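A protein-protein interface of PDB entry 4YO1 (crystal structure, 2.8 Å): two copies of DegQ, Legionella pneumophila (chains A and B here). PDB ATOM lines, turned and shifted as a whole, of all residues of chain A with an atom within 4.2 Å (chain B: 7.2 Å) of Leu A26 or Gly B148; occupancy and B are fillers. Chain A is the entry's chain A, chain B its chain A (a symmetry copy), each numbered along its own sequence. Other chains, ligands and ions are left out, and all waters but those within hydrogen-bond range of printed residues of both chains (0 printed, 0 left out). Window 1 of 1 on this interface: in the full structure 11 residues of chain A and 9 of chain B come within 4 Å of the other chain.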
ATOM      1  N   SER A  21       9.164  17.634 -20.651  1.00  0.00           N
ATOM      2  CA  SER A  21       8.987  18.013 -19.261  1.00  0.00           C
ATOM      3  C   SER A  21      10.324  18.390 -18.648  1.00  0.00           C
ATOM      4  O   SER A  21      11.337  18.498 -19.340  1.00  0.00           O
ATOM      5  CB  SER A  21       8.311  16.895 -18.458  1.00  0.00           C
ATOM      6  OG  SER A  21       6.925  16.827 -18.762  1.00  0.00           O
ATOM      7  N   LEU A  22      10.316  18.594 -17.341  1.00  0.00           N
ATOM      8  CA  LEU A  22      11.488  19.094 -16.657  1.00  0.00           C
ATOM      9  C   LEU A  22      11.944  18.077 -15.625  1.00  0.00           C
ATOM     10  O   LEU A  22      13.011  18.215 -15.026  1.00  0.00           O
ATOM     11  CB  LEU A  22      11.162  20.441 -16.020  1.00  0.00           C
ATOM     12  CG  LEU A  22      10.763  21.536 -17.020  1.00  0.00           C
ATOM     13  CD1 LEU A  22      10.255  22.779 -16.324  1.00  0.00           C
ATOM     14  CD2 LEU A  22      11.931  21.897 -17.927  1.00  0.00           C
ATOM     15  N   ALA A  23      11.118  17.051 -15.435  1.00  0.00           N
ATOM     16  CA  ALA A  23      11.440  15.939 -14.548  1.00  0.00           C
ATOM     17  C   ALA A  23      12.865  15.396 -14.718  1.00  0.00           C
ATOM     18  O   ALA A  23      13.567  15.239 -13.722  1.00  0.00           O
ATOM     19  CB  ALA A  23      10.401  14.816 -14.667  1.00  0.00           C
ATOM     20  N   PRO A  24      13.298  15.116 -15.967  1.00  0.00           N
ATOM     21  CA  PRO A  24      14.668  14.624 -16.161  1.00  0.00           C
ATOM     22  C   PRO A  24      15.704  15.507 -15.482  1.00  0.00           C
ATOM     23  O   PRO A  24      16.632  15.046 -14.817  1.00  0.00           O
ATOM     24  CB  PRO A  24      14.858  14.742 -17.677  1.00  0.00           C
ATOM     25  CG  PRO A  24      13.527  14.567 -18.226  1.00  0.00           C
ATOM     26  CD  PRO A  24      12.576  15.192 -17.252  1.00  0.00           C
ATOM     27  N   VAL A  25      15.519  16.802 -15.644  1.00  0.00           N
ATOM     28  CA  VAL A  25      16.537  17.741 -15.261  1.00  0.00           C
ATOM     29  C   VAL A  25      16.374  18.181 -13.813  1.00  0.00           C
ATOM     30  O   VAL A  25      17.317  18.672 -13.192  1.00  0.00           O
ATOM     31  CB  VAL A  25      16.517  18.929 -16.214  1.00  0.00           C
ATOM     32  CG1 VAL A  25      17.503  20.018 -15.775  1.00  0.00           C
ATOM     33  CG2 VAL A  25      16.786  18.458 -17.617  1.00  0.00           C
ATOM     34  N   LEU A  26      15.177  17.997 -13.269  1.00  0.00           N
ATOM     35  CA  LEU A  26      14.944  18.332 -11.876  1.00  0.00           C
ATOM     36  C   LEU A  26      15.434  17.203 -10.992  1.00  0.00           C
ATOM     37  O   LEU A  26      15.835  17.416  -9.845  1.00  0.00           O
ATOM     38  CB  LEU A  26      13.465  18.602 -11.633  1.00  0.00           C
ATOM     39  CG  LEU A  26      12.928  19.883 -12.278  1.00  0.00           C
ATOM     40  CD1 LEU A  26      11.592  20.262 -11.674  1.00  0.00           C
ATOM     41  CD2 LEU A  26      13.936  21.027 -12.154  1.00  0.00           C
ATOM     42  N   LYS A  27      15.394  15.995 -11.545  1.00  0.00           N
ATOM     43  CA  LYS A  27      15.931  14.812 -10.878  1.00  0.00           C
ATOM     44  C   LYS A  27      17.383  15.065 -10.529  1.00  0.00           C
ATOM     45  O   LYS A  27      17.837  14.795  -9.423  1.00  0.00           O
ATOM     46  CB  LYS A  27      15.820  13.591 -11.797  1.00  0.00           C
ATOM     47  CG  LYS A  27      15.001  12.448 -11.224  1.00  0.00           C
ATOM     48  CD  LYS A  27      14.462  11.559 -12.334  1.00  0.00           C
ATOM     49  CE  LYS A  27      13.727  10.354 -11.770  1.00  0.00           C
ATOM     50  NZ  LYS A  27      13.121   9.512 -12.843  1.00  0.00           N
ATOM     51  N   ASN A  28      18.098  15.624 -11.489  1.00  0.00           N
ATOM     52  CA  ASN A  28      19.504  15.911 -11.316  1.00  0.00           C
ATOM     53  C   ASN A  28      19.781  17.075 -10.362  1.00  0.00           C
ATOM     54  O   ASN A  28      20.747  17.053  -9.609  1.00  0.00           O
ATOM     55  CB  ASN A  28      20.120  16.159 -12.684  1.00  0.00           C
ATOM     56  CG  ASN A  28      19.747  15.077 -13.687  1.00  0.00           C
ATOM     57  OD1 ASN A  28      19.446  15.361 -14.849  1.00  0.00           O
ATOM     58  ND2 ASN A  28      19.759  13.825 -13.236  1.00  0.00           N
ATOM     59  N   ALA A  29      18.930  18.090 -10.394  1.00  0.00           N
ATOM     60  CA  ALA A  29      19.070  19.217  -9.483  1.00  0.00           C
ATOM     61  C   ALA A  29      18.786  18.827  -8.038  1.00  0.00           C
ATOM     62  O   ALA A  29      19.554  19.178  -7.151  1.00  0.00           O
ATOM     63  CB  ALA A  29      18.165  20.344  -9.905  1.00  0.00           C
ATOM     64  N   MET A  30      17.694  18.094  -7.814  1.00  0.00           N
ATOM     65  CA  MET A  30      17.225  17.741  -6.461  1.00  0.00           C
ATOM     66  C   MET A  30      18.251  17.470  -5.345  1.00  0.00           C
ATOM     67  O   MET A  30      18.169  18.107  -4.295  1.00  0.00           O
ATOM     68  CB  MET A  30      16.203  16.595  -6.495  1.00  0.00           C
ATOM     69  CG  MET A  30      14.826  17.007  -6.955  1.00  0.00           C
ATOM     70  SD  MET A  30      14.562  18.746  -6.633  1.00  0.00           S
ATOM     71  CE  MET A  30      13.903  19.262  -8.217  1.00  0.00           C
ATOM     72  N   VAL A 152      12.828  27.556 -13.017  1.00  0.00           N
ATOM     73  CA  VAL A 152      12.157  26.791 -11.974  1.00  0.00           C
ATOM     74  C   VAL A 152      12.752  27.029 -10.589  1.00  0.00           C
ATOM     75  O   VAL A 152      13.957  26.898 -10.384  1.00  0.00           O
ATOM     76  CB  VAL A 152      12.138  25.290 -12.296  1.00  0.00           C
ATOM     77  CG1 VAL A 152      11.958  24.449 -11.017  1.00  0.00           C
ATOM     78  CG2 VAL A 152      11.038  24.981 -13.305  1.00  0.00           C
ATOM     79  N   ILE A 154      13.183  25.787  -7.006  1.00  0.00           N
ATOM     80  CA  ILE A 154      13.116  24.577  -6.186  1.00  0.00           C
ATOM     81  C   ILE A 154      13.445  24.862  -4.728  1.00  0.00           C
ATOM     82  O   ILE A 154      14.198  25.789  -4.418  1.00  0.00           O
ATOM     83  CB  ILE A 154      14.112  23.514  -6.656  1.00  0.00           C
ATOM     84  CG1 ILE A 154      14.182  23.468  -8.173  1.00  0.00           C
ATOM     85  CG2 ILE A 154      13.743  22.148  -6.092  1.00  0.00           C
ATOM     86  CD1 ILE A 154      15.368  22.664  -8.640  1.00  0.00           C
ATOM     87  N   ALA A 169       8.768  22.577  -6.472  1.00  0.00           N
ATOM     88  CA  ALA A 169       9.224  23.332  -7.637  1.00  0.00           C
ATOM     89  C   ALA A 169       8.104  24.065  -8.367  1.00  0.00           C
ATOM     90  O   ALA A 169       7.049  23.503  -8.649  1.00  0.00           O
ATOM     91  CB  ALA A 169       9.947  22.423  -8.594  1.00  0.00           C
ATOM     92  N   GLU B 146       5.591  12.823 -12.600  1.00  0.00           N
ATOM     93  CA  GLU B 146       6.757  13.288 -11.860  1.00  0.00           C
ATOM     94  C   GLU B 146       6.734  14.808 -11.742  1.00  0.00           C
ATOM     95  O   GLU B 146       6.232  15.496 -12.620  1.00  0.00           O
ATOM     96  CB  GLU B 146       8.043  12.870 -12.571  1.00  0.00           C
ATOM     97  CG  GLU B 146       8.322  11.384 -12.576  1.00  0.00           C
ATOM     98  CD  GLU B 146       9.705  11.065 -13.118  1.00  0.00           C
ATOM     99  OE1 GLU B 146       9.812  10.772 -14.331  1.00  0.00           O
ATOM    100  OE2 GLU B 146      10.689  11.117 -12.341  1.00  0.00           O
ATOM    101  N   VAL B 147       7.299  15.324 -10.662  1.00  0.00           N
ATOM    102  CA  VAL B 147       7.407  16.759 -10.490  1.00  0.00           C
ATOM    103  C   VAL B 147       8.247  17.344 -11.633  1.00  0.00           C
ATOM    104  O   VAL B 147       9.279  16.787 -12.013  1.00  0.00           O
ATOM    105  CB  VAL B 147       7.950  17.122  -9.076  1.00  0.00           C
ATOM    106  CG1 VAL B 147       8.258  15.861  -8.290  1.00  0.00           C
ATOM    107  CG2 VAL B 147       9.165  18.017  -9.170  1.00  0.00           C
ATOM    108  N   GLY B 148       7.764  18.438 -12.212  1.00  0.00           N
ATOM    109  CA  GLY B 148       8.382  19.002 -13.399  1.00  0.00           C
ATOM    110  C   GLY B 148       7.541  18.812 -14.644  1.00  0.00           C
ATOM    111  O   GLY B 148       7.683  19.544 -15.619  1.00  0.00           O
ATOM    112  N   ASP B 149       6.673  17.808 -14.619  1.00  0.00           N
ATOM    113  CA  ASP B 149       5.740  17.570 -15.704  1.00  0.00           C
ATOM    114  C   ASP B 149       4.829  18.775 -15.832  1.00  0.00           C
ATOM    115  O   ASP B 149       4.353  19.293 -14.830  1.00  0.00           O
ATOM    116  CB  ASP B 149       4.893  16.328 -15.416  1.00  0.00           C
ATOM    117  CG  ASP B 149       5.661  15.036 -15.599  1.00  0.00           C
ATOM    118  OD1 ASP B 149       6.566  14.983 -16.456  1.00  0.00           O
ATOM    119  OD2 ASP B 149       5.355  14.060 -14.892  1.00  0.00           O
ATOM    120  N   TYR B 150       4.591  19.228 -17.061  1.00  0.00           N
ATOM    121  CA  TYR B 150       3.664  20.325 -17.290  1.00  0.00           C
ATOM    122  C   TYR B 150       2.261  19.829 -17.028  1.00  0.00           C
ATOM    123  O   TYR B 150       2.006  18.636 -17.006  1.00  0.00           O
ATOM    124  CB  TYR B 150       3.780  20.868 -18.717  1.00  0.00           C
ATOM    125  CG  TYR B 150       5.147  21.417 -19.035  1.00  0.00           C
ATOM    126  CD1 TYR B 150       5.605  22.572 -18.427  1.00  0.00           C
ATOM    127  CD2 TYR B 150       5.981  20.771 -19.934  1.00  0.00           C
ATOM    128  CE1 TYR B 150       6.863  23.062 -18.708  1.00  0.00           C
ATOM    129  CE2 TYR B 150       7.223  21.251 -20.222  1.00  0.00           C
ATOM    130  CZ  TYR B 150       7.666  22.392 -19.612  1.00  0.00           C
ATOM    131  OH  TYR B 150       8.920  22.870 -19.911  1.00  0.00           O
ATOM    132  N   VAL B 151       1.337  20.755 -16.853  1.00  0.00           N
ATOM    133  CA  VAL B 151       0.042  20.409 -16.297  1.00  0.00           C
ATOM    134  C   VAL B 151      -0.968  21.529 -16.530  1.00  0.00           C
ATOM    135  O   VAL B 151      -0.619  22.706 -16.442  1.00  0.00           O
ATOM    136  CB  VAL B 151       0.216  20.095 -14.796  1.00  0.00           C
ATOM    137  CG1 VAL B 151      -0.515  21.097 -13.915  1.00  0.00           C
ATOM    138  CG2 VAL B 151      -0.167  18.662 -14.515  1.00  0.00           C
ATOM    139  N   GLY B 172       0.680  25.165 -15.509  1.00  0.00           N
ATOM    140  CA  GLY B 172       1.686  25.105 -14.471  1.00  0.00           C
ATOM    141  C   GLY B 172       2.385  23.771 -14.544  1.00  0.00           C
ATOM    142  O   GLY B 172       2.235  23.044 -15.529  1.00  0.00           O
ATOM    143  N   ILE B 173       3.147  23.441 -13.507  1.00  0.00           N
ATOM    144  CA  ILE B 173       3.756  22.123 -13.413  1.00  0.00           C
ATOM    145  C   ILE B 173       3.354  21.428 -12.125  1.00  0.00           C
ATOM    146  O   ILE B 173       2.697  22.025 -11.263  1.00  0.00           O
ATOM    147  CB  ILE B 173       5.286  22.205 -13.455  1.00  0.00           C
ATOM    148  CG1 ILE B 173       5.816  22.984 -12.250  1.00  0.00           C
ATOM    149  CG2 ILE B 173       5.754  22.828 -14.768  1.00  0.00           C
ATOM    150  CD1 ILE B 173       7.321  23.004 -12.169  1.00  0.00           C
ATOM    151  N   VAL B 174       3.760  20.167 -11.995  1.00  0.00           N
ATOM    152  CA  VAL B 174       3.606  19.434 -10.744  1.00  0.00           C
ATOM    153  C   VAL B 174       4.713  19.859  -9.784  1.00  0.00           C
ATOM    154  O   VAL B 174       5.900  19.797 -10.132  1.00  0.00           O
ATOM    155  CB  VAL B 174       3.665  17.928 -10.982  1.00  0.00           C
ATOM    156  CG1 VAL B 174       3.758  17.188  -9.673  1.00  0.00           C
ATOM    157  CG2 VAL B 174       2.443  17.475 -11.778  1.00  0.00           C
ATOM    158  N   SER B 175       4.318  20.303  -8.592  1.00  0.00           N
ATOM    159  CA  SER B 175       5.234  20.899  -7.628  1.00  0.00           C
ATOM    160  C   SER B 175       5.806  19.895  -6.642  1.00  0.00           C
ATOM    161  O   SER B 175       6.958  20.003  -6.225  1.00  0.00           O
ATOM    162  CB  SER B 175       4.505  21.975  -6.836  1.00  0.00           C
ATOM    163  OG  SER B 175       4.538  23.217  -7.508  1.00  0.00           O
ATOM    164  N   ALA B 176       4.978  18.929  -6.256  1.00  0.00           N
ATOM    165  CA  ALA B 176       5.365  17.895  -5.310  1.00  0.00           C
ATOM    166  C   ALA B 176       4.422  16.703  -5.454  1.00  0.00           C
ATOM    167  O   ALA B 176       3.365  16.811  -6.078  1.00  0.00           O
ATOM    168  CB  ALA B 176       5.317  18.445  -3.904  1.00  0.00           C
ATOM    169  N   LEU B 177       4.806  15.565  -4.886  1.00  0.00           N
ATOM    170  CA  LEU B 177       3.966  14.369  -4.927  1.00  0.00           C
ATOM    171  C   LEU B 177       3.957  13.657  -3.573  1.00  0.00           C
ATOM    172  O   LEU B 177       2.898  13.447  -2.973  1.00  0.00           O
ATOM    173  CB  LEU B 177       4.428  13.412  -6.033  1.00  0.00           C
ATOM    174  CG  LEU B 177       4.321  13.932  -7.468  1.00  0.00           C
ATOM    175  CD1 LEU B 177       5.089  13.045  -8.419  1.00  0.00           C
ATOM    176  CD2 LEU B 177       2.868  14.046  -7.905  1.00  0.00           C
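O of Gly B148 lies within hydrogen-bond range of N of Leu A22 (3.3 Å). The side-chain hydroxyl of Ser A21 lies within hydrogen-bond range of the side-chain carboxylate of Asp B149 (3.0 Å). The side-chain amino group (NZ) of Lys A27 is in salt-bridge range of the side-chain carboxylate (OE2) of Glu B146 (3.0 Å). O of Ala A169 sits at hydrogen-bond distance from OG of Ser B175 (2.8 Å).
The backbone NH of Val B174 lies within hydrogen-bond range of the backbone carbonyl oxygen of Asp B149, 3.0 Å away. OD2 of Asp B149 lies within hydrogen-bond range of N of Glu B146 (2.6 Å). N of Gly B148 lies within hydrogen-bond range of O of Val B174, at 3.1 Å.
Among the printed residues, merely in contact across the chains: Ser A21 with Gly B148 (3.9 Å), Ser A21 with Tyr B150 (3.8 Å), Leu A22 with Tyr B150 (3.7 Å), Ala A23 with Glu B146 (3.7 Å), Ala A23 with Val B147 (3.4 Å), Ala A23 with Gly B148 (3.9 Å), Leu A26 with Gly B148 (3.9 Å) and Ala A169 with Ile B173 (3.6 Å).
Of chain B, only Gly B148 comes within 4 Å of Leu A26. Gly B148 touches four residues of chain A. Printed residues of chain B within 4 Å of Ser A21: Gly B148 (3.9 Å), Asp B149 (3.0 Å) and Tyr B150 (3.8 Å). Of the printed residues of chain A, Tyr B150 touches Ser A21 (3.8 Å) and Leu A22 (3.7 Å). Pro A24 touches none of the printed residues of chain B. Ala B176 touches none of the printed residues of chain A. The nearest residue of chain B that does not touch Leu A26 is Val B147 (4.1 Å). The nearest printed residue of chain A that does not touch Gly B148 is Ala A169 (5.8 Å).
Hydrophobic or aromatic side chains of chain B within 4 Å of the printed part of chain A: Tyr B150 and Ile B173. Hydrophobic or aromatic side chains of chain A that line the printed part of chain B: Leu A22, Ala A23 and Leu A26. Among the printed residues, 12 pairs touch across the chains.
No position is printed for both chains.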
